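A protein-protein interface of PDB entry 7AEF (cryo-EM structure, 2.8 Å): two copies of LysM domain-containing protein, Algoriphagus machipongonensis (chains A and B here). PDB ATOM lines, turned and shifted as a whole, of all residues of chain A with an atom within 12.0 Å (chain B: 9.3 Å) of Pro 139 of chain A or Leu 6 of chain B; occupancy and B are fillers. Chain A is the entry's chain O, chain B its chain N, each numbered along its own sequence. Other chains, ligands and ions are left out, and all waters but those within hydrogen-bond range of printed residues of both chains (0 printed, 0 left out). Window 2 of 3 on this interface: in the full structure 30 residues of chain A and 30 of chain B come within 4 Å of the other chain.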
ATOM      1  N   ARG A  76     -31.553  16.193 -30.833  1.00  0.00           N
ATOM      2  CA  ARG A  76     -32.676  16.300 -29.902  1.00  0.00           C
ATOM      3  C   ARG A  76     -33.210  17.727 -29.884  1.00  0.00           C
ATOM      4  O   ARG A  76     -33.329  18.363 -28.839  1.00  0.00           O
ATOM      5  CB  ARG A  76     -32.310  15.864 -28.480  1.00  0.00           C
ATOM      6  CG  ARG A  76     -31.786  14.435 -28.336  1.00  0.00           C
ATOM      7  CD  ARG A  76     -32.763  13.376 -28.790  1.00  0.00           C
ATOM      8  NE  ARG A  76     -33.925  13.212 -27.929  1.00  0.00           N
ATOM      9  CZ  ARG A  76     -34.020  12.295 -26.974  1.00  0.00           C
ATOM     10  NH1 ARG A  76     -33.021  11.455 -26.752  1.00  0.00           N
ATOM     11  NH2 ARG A  76     -35.119  12.214 -26.245  1.00  0.00           N
ATOM     12  N   THR A  77     -33.511  18.262 -31.064  1.00  0.00           N
ATOM     13  CA  THR A  77     -34.055  19.607 -31.215  1.00  0.00           C
ATOM     14  C   THR A  77     -35.581  19.640 -31.103  1.00  0.00           C
ATOM     15  O   THR A  77     -36.128  20.544 -30.463  1.00  0.00           O
ATOM     16  CB  THR A  77     -33.578  20.195 -32.551  1.00  0.00           C
ATOM     17  OG1 THR A  77     -32.162  20.392 -32.492  1.00  0.00           O
ATOM     18  CG2 THR A  77     -34.229  21.521 -32.866  1.00  0.00           C
ATOM     19  N   THR A  86     -35.236  16.384 -24.373  1.00  0.00           N
ATOM     20  CA  THR A  86     -34.708  15.980 -23.084  1.00  0.00           C
ATOM     21  C   THR A  86     -34.112  17.216 -22.421  1.00  0.00           C
ATOM     22  O   THR A  86     -33.778  18.189 -23.095  1.00  0.00           O
ATOM     23  CB  THR A  86     -33.660  14.871 -23.275  1.00  0.00           C
ATOM     24  OG1 THR A  86     -34.145  13.937 -24.243  1.00  0.00           O
ATOM     25  CG2 THR A  86     -33.457  14.079 -22.002  1.00  0.00           C
ATOM     26  N   GLU A  87     -34.036  17.192 -21.086  1.00  0.00           N
ATOM     27  CA  GLU A  87     -33.477  18.323 -20.349  1.00  0.00           C
ATOM     28  C   GLU A  87     -31.995  18.521 -20.642  1.00  0.00           C
ATOM     29  O   GLU A  87     -31.521  19.660 -20.703  1.00  0.00           O
ATOM     30  CB  GLU A  87     -33.713  18.128 -18.848  1.00  0.00           C
ATOM     31  CG  GLU A  87     -33.164  19.242 -17.962  1.00  0.00           C
ATOM     32  CD  GLU A  87     -33.853  20.577 -18.180  1.00  0.00           C
ATOM     33  OE1 GLU A  87     -35.057  20.593 -18.510  1.00  0.00           O
ATOM     34  OE2 GLU A  87     -33.180  21.620 -18.036  1.00  0.00           O
ATOM     35  N   ASP A  88     -31.256  17.440 -20.864  1.00  0.00           N
ATOM     36  CA  ASP A  88     -29.826  17.548 -21.101  1.00  0.00           C
ATOM     37  C   ASP A  88     -29.418  17.252 -22.539  1.00  0.00           C
ATOM     38  O   ASP A  88     -28.229  17.060 -22.795  1.00  0.00           O
ATOM     39  CB  ASP A  88     -29.065  16.642 -20.132  1.00  0.00           C
ATOM     40  CG  ASP A  88     -29.520  15.206 -20.188  1.00  0.00           C
ATOM     41  OD1 ASP A  88     -30.498  14.910 -20.891  1.00  0.00           O
ATOM     42  OD2 ASP A  88     -28.891  14.361 -19.520  1.00  0.00           O
ATOM     43  N   GLY A  89     -30.359  17.212 -23.478  1.00  0.00           N
ATOM     44  CA  GLY A  89     -29.984  17.134 -24.882  1.00  0.00           C
ATOM     45  C   GLY A  89     -29.449  15.773 -25.274  1.00  0.00           C
ATOM     46  O   GLY A  89     -30.092  14.742 -25.061  1.00  0.00           O
ATOM     47  N   ILE A  91     -26.443  14.529 -24.213  1.00  0.00           N
ATOM     48  CA  ILE A  91     -25.314  14.216 -23.335  1.00  0.00           C
ATOM     49  C   ILE A  91     -25.318  12.740 -22.953  1.00  0.00           C
ATOM     50  O   ILE A  91     -24.278  12.071 -22.975  1.00  0.00           O
ATOM     51  CB  ILE A  91     -25.330  15.129 -22.091  1.00  0.00           C
ATOM     52  CG1 ILE A  91     -25.023  16.571 -22.477  1.00  0.00           C
ATOM     53  CG2 ILE A  91     -24.316  14.686 -21.064  1.00  0.00           C
ATOM     54  CD1 ILE A  91     -25.272  17.573 -21.361  1.00  0.00           C
ATOM     55  N   LYS A 135     -22.204  20.518 -32.987  1.00  0.00           N
ATOM     56  CA  LYS A 135     -22.689  21.511 -33.944  1.00  0.00           C
ATOM     57  C   LYS A 135     -23.578  22.597 -33.352  1.00  0.00           C
ATOM     58  O   LYS A 135     -23.297  23.777 -33.557  1.00  0.00           O
ATOM     59  CB  LYS A 135     -23.453  20.818 -35.076  1.00  0.00           C
ATOM     60  CG  LYS A 135     -22.650  19.860 -35.915  1.00  0.00           C
ATOM     61  CD  LYS A 135     -23.584  19.104 -36.847  1.00  0.00           C
ATOM     62  CE  LYS A 135     -22.833  18.347 -37.922  1.00  0.00           C
ATOM     63  NZ  LYS A 135     -21.748  19.166 -38.522  1.00  0.00           N
ATOM     64  N   LEU A 136     -24.665  22.247 -32.662  1.00  0.00           N
ATOM     65  CA  LEU A 136     -25.569  23.224 -32.059  1.00  0.00           C
ATOM     66  C   LEU A 136     -25.556  23.122 -30.545  1.00  0.00           C
ATOM     67  O   LEU A 136     -25.333  22.054 -29.978  1.00  0.00           O
ATOM     68  CB  LEU A 136     -27.023  23.061 -32.506  1.00  0.00           C
ATOM     69  CG  LEU A 136     -27.659  23.645 -33.755  1.00  0.00           C
ATOM     70  CD1 LEU A 136     -29.104  23.234 -33.727  1.00  0.00           C
ATOM     71  CD2 LEU A 136     -27.556  25.145 -33.751  1.00  0.00           C
ATOM     72  N   PHE A 137     -25.835  24.254 -29.898  1.00  0.00           N
ATOM     73  CA  PHE A 137     -25.801  24.375 -28.451  1.00  0.00           C
ATOM     74  C   PHE A 137     -26.974  25.218 -27.968  1.00  0.00           C
ATOM     75  O   PHE A 137     -27.437  26.126 -28.655  1.00  0.00           O
ATOM     76  CB  PHE A 137     -24.483  25.009 -27.959  1.00  0.00           C
ATOM     77  CG  PHE A 137     -23.252  24.323 -28.472  1.00  0.00           C
ATOM     78  CD1 PHE A 137     -22.634  24.750 -29.640  1.00  0.00           C
ATOM     79  CD2 PHE A 137     -22.712  23.250 -27.793  1.00  0.00           C
ATOM     80  CE1 PHE A 137     -21.521  24.108 -30.118  1.00  0.00           C
ATOM     81  CE2 PHE A 137     -21.597  22.612 -28.266  1.00  0.00           C
ATOM     82  CZ  PHE A 137     -21.003  23.039 -29.427  1.00  0.00           C
ATOM     83  N   ARG A 138     -27.441  24.898 -26.768  1.00  0.00           N
ATOM     84  CA  ARG A 138     -28.311  25.775 -26.002  1.00  0.00           C
ATOM     85  C   ARG A 138     -27.488  26.943 -25.453  1.00  0.00           C
ATOM     86  O   ARG A 138     -26.261  26.856 -25.405  1.00  0.00           O
ATOM     87  CB  ARG A 138     -28.965  24.973 -24.881  1.00  0.00           C
ATOM     88  CG  ARG A 138     -30.270  24.323 -25.257  1.00  0.00           C
ATOM     89  CD  ARG A 138     -30.841  23.636 -24.052  1.00  0.00           C
ATOM     90  NE  ARG A 138     -31.683  22.502 -24.405  1.00  0.00           N
ATOM     91  CZ  ARG A 138     -31.923  21.475 -23.596  1.00  0.00           C
ATOM     92  NH1 ARG A 138     -31.383  21.443 -22.386  1.00  0.00           N
ATOM     93  NH2 ARG A 138     -32.699  20.483 -23.997  1.00  0.00           N
ATOM     94  N   PRO A 139     -28.140  28.068 -25.069  1.00  0.00           N
ATOM     95  CA  PRO A 139     -27.391  29.227 -24.537  1.00  0.00           C
ATOM     96  C   PRO A 139     -26.502  28.968 -23.328  1.00  0.00           C
ATOM     97  O   PRO A 139     -25.509  29.680 -23.147  1.00  0.00           O
ATOM     98  CB  PRO A 139     -28.507  30.211 -24.176  1.00  0.00           C
ATOM     99  CG  PRO A 139     -29.575  29.915 -25.107  1.00  0.00           C
ATOM    100  CD  PRO A 139     -29.525  28.455 -25.405  1.00  0.00           C
ATOM    101  N   ASP A 140     -26.801  27.957 -22.515  1.00  0.00           N
ATOM    102  CA  ASP A 140     -25.971  27.627 -21.367  1.00  0.00           C
ATOM    103  C   ASP A 140     -24.905  26.589 -21.701  1.00  0.00           C
ATOM    104  O   ASP A 140     -24.221  26.097 -20.805  1.00  0.00           O
ATOM    105  CB  ASP A 140     -26.831  27.157 -20.195  1.00  0.00           C
ATOM    106  CG  ASP A 140     -27.595  25.899 -20.496  1.00  0.00           C
ATOM    107  OD1 ASP A 140     -27.974  25.698 -21.661  1.00  0.00           O
ATOM    108  OD2 ASP A 140     -27.839  25.117 -19.561  1.00  0.00           O
ATOM    109  N   GLY A 141     -24.749  26.251 -22.977  1.00  0.00           N
ATOM    110  CA  GLY A 141     -23.704  25.352 -23.414  1.00  0.00           C
ATOM    111  C   GLY A 141     -24.067  23.886 -23.443  1.00  0.00           C
ATOM    112  O   GLY A 141     -23.167  23.048 -23.368  1.00  0.00           O
ATOM    113  N   THR A 142     -25.337  23.551 -23.532  1.00  0.00           N
ATOM    114  CA  THR A 142     -25.745  22.158 -23.662  1.00  0.00           C
ATOM    115  C   THR A 142     -25.851  21.789 -25.136  1.00  0.00           C
ATOM    116  O   THR A 142     -26.570  22.458 -25.878  1.00  0.00           O
ATOM    117  CB  THR A 142     -27.083  21.934 -22.974  1.00  0.00           C
ATOM    118  OG1 THR A 142     -27.060  22.551 -21.684  1.00  0.00           O
ATOM    119  CG2 THR A 142     -27.367  20.464 -22.813  1.00  0.00           C
ATOM    120  N   PRO A 143     -25.169  20.740 -25.596  1.00  0.00           N
ATOM    121  CA  PRO A 143     -25.215  20.403 -27.025  1.00  0.00           C
ATOM    122  C   PRO A 143     -26.484  19.657 -27.405  1.00  0.00           C
ATOM    123  O   PRO A 143     -27.012  18.853 -26.637  1.00  0.00           O
ATOM    124  CB  PRO A 143     -23.976  19.523 -27.212  1.00  0.00           C
ATOM    125  CG  PRO A 143     -23.754  18.917 -25.886  1.00  0.00           C
ATOM    126  CD  PRO A 143     -24.179  19.930 -24.871  1.00  0.00           C
ATOM    127  N   ILE A 144     -26.979  19.932 -28.612  1.00  0.00           N
ATOM    128  CA  ILE A 144     -28.212  19.321 -29.089  1.00  0.00           C
ATOM    129  C   ILE A 144     -28.053  18.689 -30.465  1.00  0.00           C
ATOM    130  O   ILE A 144     -29.013  18.114 -30.988  1.00  0.00           O
ATOM    131  CB  ILE A 144     -29.374  20.339 -29.087  1.00  0.00           C
ATOM    132  CG1 ILE A 144     -28.938  21.669 -29.691  1.00  0.00           C
ATOM    133  CG2 ILE A 144     -29.912  20.552 -27.687  1.00  0.00           C
ATOM    134  CD1 ILE A 144     -30.044  22.666 -29.817  1.00  0.00           C
ATOM    135  N   ARG A 145     -26.861  18.763 -31.064  1.00  0.00           N
ATOM    136  CA  ARG A 145     -26.615  18.111 -32.347  1.00  0.00           C
ATOM    137  C   ARG A 145     -25.144  17.737 -32.547  1.00  0.00           C
ATOM    138  O   ARG A 145     -24.254  18.535 -32.263  1.00  0.00           O
ATOM    139  CB  ARG A 145     -27.085  18.997 -33.501  1.00  0.00           C
ATOM    140  CG  ARG A 145     -27.444  18.215 -34.746  1.00  0.00           C
ATOM    141  CD  ARG A 145     -27.863  19.116 -35.876  1.00  0.00           C
ATOM    142  NE  ARG A 145     -29.232  19.587 -35.716  1.00  0.00           N
ATOM    143  CZ  ARG A 145     -29.676  20.743 -36.188  1.00  0.00           C
ATOM    144  NH1 ARG A 145     -28.859  21.547 -36.846  1.00  0.00           N
ATOM    145  NH2 ARG A 145     -30.934  21.094 -35.998  1.00  0.00           N
ATOM    146  N   SER B   2     -31.215  30.962 -14.431  1.00  0.00           N
ATOM    147  CA  SER B   2     -29.968  31.253 -15.124  1.00  0.00           C
ATOM    148  C   SER B   2     -29.804  30.376 -16.354  1.00  0.00           C
ATOM    149  O   SER B   2     -28.694  30.174 -16.836  1.00  0.00           O
ATOM    150  CB  SER B   2     -28.778  31.066 -14.183  1.00  0.00           C
ATOM    151  OG  SER B   2     -27.567  30.957 -14.908  1.00  0.00           O
ATOM    152  N   GLU B   3     -30.926  29.831 -16.819  1.00  0.00           N
ATOM    153  CA  GLU B   3     -30.975  29.123 -18.090  1.00  0.00           C
ATOM    154  C   GLU B   3     -30.750  30.087 -19.242  1.00  0.00           C
ATOM    155  O   GLU B   3     -30.080  29.758 -20.226  1.00  0.00           O
ATOM    156  CB  GLU B   3     -32.327  28.429 -18.257  1.00  0.00           C
ATOM    157  CG  GLU B   3     -32.433  27.580 -19.508  1.00  0.00           C
ATOM    158  CD  GLU B   3     -33.765  26.864 -19.627  1.00  0.00           C
ATOM    159  OE1 GLU B   3     -34.041  26.283 -20.697  1.00  0.00           O
ATOM    160  OE2 GLU B   3     -34.573  26.961 -18.680  1.00  0.00           O
ATOM    161  N   GLY B   4     -31.317  31.286 -19.116  1.00  0.00           N
ATOM    162  CA  GLY B   4     -31.281  32.301 -20.141  1.00  0.00           C
ATOM    163  C   GLY B   4     -29.952  32.985 -20.319  1.00  0.00           C
ATOM    164  O   GLY B   4     -29.809  33.802 -21.232  1.00  0.00           O
ATOM    165  N   LYS B   5     -28.978  32.679 -19.474  1.00  0.00           N
ATOM    166  CA  LYS B   5     -27.650  33.263 -19.576  1.00  0.00           C
ATOM    167  C   LYS B   5     -26.827  32.559 -20.644  1.00  0.00           C
ATOM    168  O   LYS B   5     -26.733  31.331 -20.655  1.00  0.00           O
ATOM    169  CB  LYS B   5     -26.933  33.174 -18.232  1.00  0.00           C
ATOM    170  CG  LYS B   5     -25.524  33.710 -18.264  1.00  0.00           C
ATOM    171  CD  LYS B   5     -24.717  33.242 -17.085  1.00  0.00           C
ATOM    172  CE  LYS B   5     -23.277  33.682 -17.222  1.00  0.00           C
ATOM    173  NZ  LYS B   5     -22.478  33.337 -16.018  1.00  0.00           N
ATOM    174  N   LEU B   6     -26.219  33.345 -21.530  1.00  0.00           N
ATOM    175  CA  LEU B   6     -25.253  32.844 -22.503  1.00  0.00           C
ATOM    176  C   LEU B   6     -23.912  32.645 -21.806  1.00  0.00           C
ATOM    177  O   LEU B   6     -23.229  33.615 -21.471  1.00  0.00           O
ATOM    178  CB  LEU B   6     -25.125  33.805 -23.680  1.00  0.00           C
ATOM    179  CG  LEU B   6     -24.215  33.371 -24.839  1.00  0.00           C
ATOM    180  CD1 LEU B   6     -24.761  32.148 -25.533  1.00  0.00           C
ATOM    181  CD2 LEU B   6     -24.029  34.491 -25.834  1.00  0.00           C
ATOM    182  N   GLU B   7     -23.527  31.393 -21.598  1.00  0.00           N
ATOM    183  CA  GLU B   7     -22.263  31.086 -20.946  1.00  0.00           C
ATOM    184  C   GLU B   7     -21.101  31.237 -21.923  1.00  0.00           C
ATOM    185  O   GLU B   7     -21.228  30.954 -23.115  1.00  0.00           O
ATOM    186  CB  GLU B   7     -22.303  29.665 -20.375  1.00  0.00           C
ATOM    187  CG  GLU B   7     -21.151  29.309 -19.443  1.00  0.00           C
ATOM    188  CD  GLU B   7     -21.310  29.882 -18.040  1.00  0.00           C
ATOM    189  OE1 GLU B   7     -20.308  29.927 -17.301  1.00  0.00           O
ATOM    190  OE2 GLU B   7     -22.431  30.277 -17.667  1.00  0.00           O
ATOM    191  N   LYS B   8     -19.962  31.694 -21.410  1.00  0.00           N
ATOM    192  CA  LYS B   8     -18.757  31.926 -22.192  1.00  0.00           C
ATOM    193  C   LYS B   8     -17.667  30.946 -21.782  1.00  0.00           C
ATOM    194  O   LYS B   8     -17.572  30.561 -20.614  1.00  0.00           O
ATOM    195  CB  LYS B   8     -18.276  33.363 -22.008  1.00  0.00           C
ATOM    196  CG  LYS B   8     -19.148  34.380 -22.704  1.00  0.00           C
ATOM    197  CD  LYS B   8     -18.919  34.346 -24.197  1.00  0.00           C
ATOM    198  CE  LYS B   8     -20.068  34.970 -24.940  1.00  0.00           C
ATOM    199  NZ  LYS B   8     -20.340  36.344 -24.470  1.00  0.00           N
ATOM    200  N   LEU B   9     -16.840  30.551 -22.747  1.00  0.00           N
ATOM    201  CA  LEU B   9     -15.810  29.540 -22.527  1.00  0.00           C
ATOM    202  C   LEU B   9     -14.658  30.111 -21.701  1.00  0.00           C
ATOM    203  O   LEU B   9     -14.291  31.276 -21.844  1.00  0.00           O
ATOM    204  CB  LEU B   9     -15.330  29.016 -23.884  1.00  0.00           C
ATOM    205  CG  LEU B   9     -14.044  28.229 -24.147  1.00  0.00           C
ATOM    206  CD1 LEU B   9     -13.957  27.014 -23.299  1.00  0.00           C
ATOM    207  CD2 LEU B   9     -13.995  27.806 -25.581  1.00  0.00           C
ATOM    208  N   ILE B  29     -10.981  34.323 -20.105  1.00  0.00           N
ATOM    209  CA  ILE B  29     -12.385  34.224 -20.484  1.00  0.00           C
ATOM    210  C   ILE B  29     -12.537  34.855 -21.857  1.00  0.00           C
ATOM    211  O   ILE B  29     -12.098  35.987 -22.073  1.00  0.00           O
ATOM    212  CB  ILE B  29     -13.314  34.910 -19.463  1.00  0.00           C
ATOM    213  CG1 ILE B  29     -13.053  34.395 -18.050  1.00  0.00           C
ATOM    214  CG2 ILE B  29     -14.766  34.682 -19.817  1.00  0.00           C
ATOM    215  CD1 ILE B  29     -13.600  35.271 -16.971  1.00  0.00           C
ATOM    216  N   THR B  30     -13.161  34.135 -22.781  1.00  0.00           N
ATOM    217  CA  THR B  30     -13.341  34.643 -24.130  1.00  0.00           C
ATOM    218  C   THR B  30     -14.505  35.637 -24.183  1.00  0.00           C
ATOM    219  O   THR B  30     -15.348  35.705 -23.287  1.00  0.00           O
ATOM    220  CB  THR B  30     -13.559  33.490 -25.115  1.00  0.00           C
ATOM    221  OG1 THR B  30     -13.302  33.941 -26.446  1.00  0.00           O
ATOM    222  CG2 THR B  30     -14.977  32.962 -25.047  1.00  0.00           C
ATOM    223  N   LEU B  31     -14.526  36.437 -25.243  1.00  0.00           N
ATOM    224  CA  LEU B  31     -15.633  37.351 -25.478  1.00  0.00           C
ATOM    225  C   LEU B  31     -16.585  36.862 -26.557  1.00  0.00           C
ATOM    226  O   LEU B  31     -17.731  37.313 -26.598  1.00  0.00           O
ATOM    227  CB  LEU B  31     -15.114  38.741 -25.855  1.00  0.00           C
ATOM    228  CG  LEU B  31     -14.181  39.451 -24.867  1.00  0.00           C
ATOM    229  CD1 LEU B  31     -13.318  40.451 -25.596  1.00  0.00           C
ATOM    230  CD2 LEU B  31     -14.944  40.136 -23.754  1.00  0.00           C
ATOM    231  N   LEU B  32     -16.132  35.969 -27.432  1.00  0.00           N
ATOM    232  CA  LEU B  32     -16.985  35.301 -28.403  1.00  0.00           C
ATOM    233  C   LEU B  32     -16.667  33.817 -28.394  1.00  0.00           C
ATOM    234  O   LEU B  32     -15.504  33.425 -28.457  1.00  0.00           O
ATOM    235  CB  LEU B  32     -16.796  35.866 -29.809  1.00  0.00           C
ATOM    236  CG  LEU B  32     -17.138  37.337 -30.033  1.00  0.00           C
ATOM    237  CD1 LEU B  32     -16.351  37.874 -31.206  1.00  0.00           C
ATOM    238  CD2 LEU B  32     -18.625  37.515 -30.251  1.00  0.00           C
ATOM    239  N   ASN B  33     -17.697  33.017 -28.321  1.00  0.00           N
ATOM    240  CA  ASN B  33     -17.620  31.566 -28.286  1.00  0.00           C
ATOM    241  C   ASN B  33     -17.241  31.012 -29.655  1.00  0.00           C
ATOM    242  O   ASN B  33     -17.569  31.604 -30.684  1.00  0.00           O
ATOM    243  CB  ASN B  33     -18.972  30.984 -27.870  1.00  0.00           C
ATOM    244  CG  ASN B  33     -19.136  30.902 -26.376  1.00  0.00           C
ATOM    245  OD1 ASN B  33     -18.220  30.514 -25.671  1.00  0.00           O
ATOM    246  ND2 ASN B  33     -20.305  31.271 -25.885  1.00  0.00           N
ATOM    247  N   PRO B  34     -16.551  29.872 -29.698  1.00  0.00           N
ATOM    248  CA  PRO B  34     -16.364  29.175 -30.972  1.00  0.00           C
ATOM    249  C   PRO B  34     -17.691  28.654 -31.512  1.00  0.00           C
ATOM    250  O   PRO B  34     -18.686  28.554 -30.796  1.00  0.00           O
ATOM    251  CB  PRO B  34     -15.415  28.027 -30.616  1.00  0.00           C
ATOM    252  CG  PRO B  34     -14.795  28.412 -29.341  1.00  0.00           C
ATOM    253  CD  PRO B  34     -15.795  29.233 -28.610  1.00  0.00           C
ATOM    254  N   ILE B  80     -20.459  45.046 -31.444  1.00  0.00           N
ATOM    255  CA  ILE B  80     -20.962  43.925 -30.664  1.00  0.00           C
ATOM    256  C   ILE B  80     -21.478  44.473 -29.343  1.00  0.00           C
ATOM    257  O   ILE B  80     -20.746  45.154 -28.616  1.00  0.00           O
ATOM    258  CB  ILE B  80     -19.877  42.858 -30.451  1.00  0.00           C
ATOM    259  CG1 ILE B  80     -19.503  42.240 -31.798  1.00  0.00           C
ATOM    260  CG2 ILE B  80     -20.342  41.804 -29.466  1.00  0.00           C
ATOM    261  CD1 ILE B  80     -18.631  41.017 -31.708  1.00  0.00           C
ATOM    262  N   ALA B  81     -22.739  44.179 -29.036  1.00  0.00           N
ATOM    263  CA  ALA B  81     -23.401  44.762 -27.877  1.00  0.00           C
ATOM    264  C   ALA B  81     -22.856  44.182 -26.577  1.00  0.00           C
ATOM    265  O   ALA B  81     -22.682  42.970 -26.444  1.00  0.00           O
ATOM    266  CB  ALA B  81     -24.907  44.530 -27.960  1.00  0.00           C
ATOM    267  N   TYR B  83     -19.867  45.398 -25.047  1.00  0.00           N
ATOM    268  CA  TYR B  83     -18.445  45.638 -24.879  1.00  0.00           C
ATOM    269  C   TYR B  83     -18.092  47.050 -25.315  1.00  0.00           C
ATOM    270  O   TYR B  83     -18.853  47.710 -26.025  1.00  0.00           O
ATOM    271  CB  TYR B  83     -17.620  44.623 -25.668  1.00  0.00           C
ATOM    272  CG  TYR B  83     -17.910  43.211 -25.252  1.00  0.00           C
ATOM    273  CD1 TYR B  83     -17.955  42.869 -23.911  1.00  0.00           C
ATOM    274  CD2 TYR B  83     -18.161  42.221 -26.194  1.00  0.00           C
ATOM    275  CE1 TYR B  83     -18.236  41.578 -23.509  1.00  0.00           C
ATOM    276  CE2 TYR B  83     -18.440  40.922 -25.806  1.00  0.00           C
ATOM    277  CZ  TYR B  83     -18.474  40.606 -24.461  1.00  0.00           C
ATOM    278  OH  TYR B  83     -18.749  39.322 -24.053  1.00  0.00           O
ATOM    279  N   TRP B 118     -16.670  24.636 -20.758  1.00  0.00           N
ATOM    280  CA  TRP B 118     -17.771  25.385 -21.362  1.00  0.00           C
ATOM    281  C   TRP B 118     -18.998  24.488 -21.377  1.00  0.00           C
ATOM    282  O   TRP B 118     -19.070  23.565 -22.188  1.00  0.00           O
ATOM    283  CB  TRP B 118     -17.423  25.842 -22.773  1.00  0.00           C
ATOM    284  CG  TRP B 118     -18.539  26.543 -23.490  1.00  0.00           C
ATOM    285  CD1 TRP B 118     -19.458  27.388 -22.950  1.00  0.00           C
ATOM    286  CD2 TRP B 118     -18.843  26.464 -24.883  1.00  0.00           C
ATOM    287  NE1 TRP B 118     -20.322  27.828 -23.911  1.00  0.00           N
ATOM    288  CE2 TRP B 118     -19.964  27.278 -25.110  1.00  0.00           C
ATOM    289  CE3 TRP B 118     -18.276  25.780 -25.962  1.00  0.00           C
ATOM    290  CZ2 TRP B 118     -20.536  27.425 -26.371  1.00  0.00           C
ATOM    291  CZ3 TRP B 118     -18.841  25.933 -27.213  1.00  0.00           C
ATOM    292  CH2 TRP B 118     -19.959  26.751 -27.407  1.00  0.00           C
ATOM    293  N   GLY B 119     -19.961  24.776 -20.509  1.00  0.00           N
ATOM    294  CA  GLY B 119     -21.184  23.996 -20.462  1.00  0.00           C
ATOM    295  C   GLY B 119     -20.941  22.586 -19.971  1.00  0.00           C
ATOM    296  O   GLY B 119     -20.528  22.362 -18.833  1.00  0.00           O
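Along chain A the printed residues that touch a printed residue of chain B span positions 139 to 141.
Of the 19 printed residues of chain B, 4 touch a printed residue of chain A.
Hydrophobic or aromatic side chains of chain B that line the printed part of chain A: Leu 6.
Among the printed residues, 6 pairs touch across the chains.
Among the printed residues, merely in contact across the chains: Pro 139 of chain A with Leu 6 of chain B (3.2 Å), Gly 141 of chain A with Gly 119 of chain B (3.6 Å), Asp 140 of chain A with Gly 119 of chain B (3.7 Å) and Asp 140 of chain A with Lys 5 of chain B (3.8 Å).
The side-chain amino group (NZ) of Lys 5 of chain B lies within salt-bridge range of the side-chain carboxylate (OE2) of Glu 7 of chain B, at 3.5 Å.
The side-chain amide nitrogen (ND2) of Asn 33 of chain B is in hydrogen-bond range of the backbone carbonyl oxygen (O) of Glu 7 of chain B.
The backbone carbonyl oxygen of Glu 7 of chain B lies within hydrogen-bond range of the indole nitrogen of Trp 118 of chain B.
OD1 of Asp 140 of chain A sits at hydrogen-bond distance from OG1 of Thr 142 of chain A, 3.3 Å away.
Of the printed residues of chain B, Asp 140 of chain A touches Lys 5 (3.8 Å) and Gly 119 (3.7 Å).
Printed residues of chain B within 4 Å of Gly 141 of chain A: Gly 119 (3.6 Å).
Lys 5 of chain B touches just these residues of chain A: Pro 139 and Asp 140.
Leu 6 of chain B touches just one residue of chain A: Pro 139 (3.2 Å).
Of chain A, only Pro 139 comes within 4 Å of Glu 7 of chain B.
Ile 80 of chain B touches none of the printed residues of chain A.
Printed residues of chain A within 4 Å of Gly 119 of chain B: Asp 140 (3.7 Å) and Gly 141 (3.6 Å).
The nearest residue of chain B that does not touch Pro 139 of chain A is Glu 3 of chain B (4.3 Å).
The nearest residue of chain A that does not touch Leu 6 of chain B is Asp 140 of chain A (5.1 Å).
No position is printed for both chains.
Of the 6 pairs that touch across the chains among the printed residues, none has its exchanged pair printed and touching as well.
The backbone NH (N) of Glu 7 of chain B lies within hydrogen-bond range of the backbone carbonyl oxygen (O) of Pro 139 of chain A (3.0 Å).
The backbone carbonyl oxygen of Lys 5 of chain B sits close to the backbone carbonyl oxygen of Pro 139 of chain A (3.2 Å).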
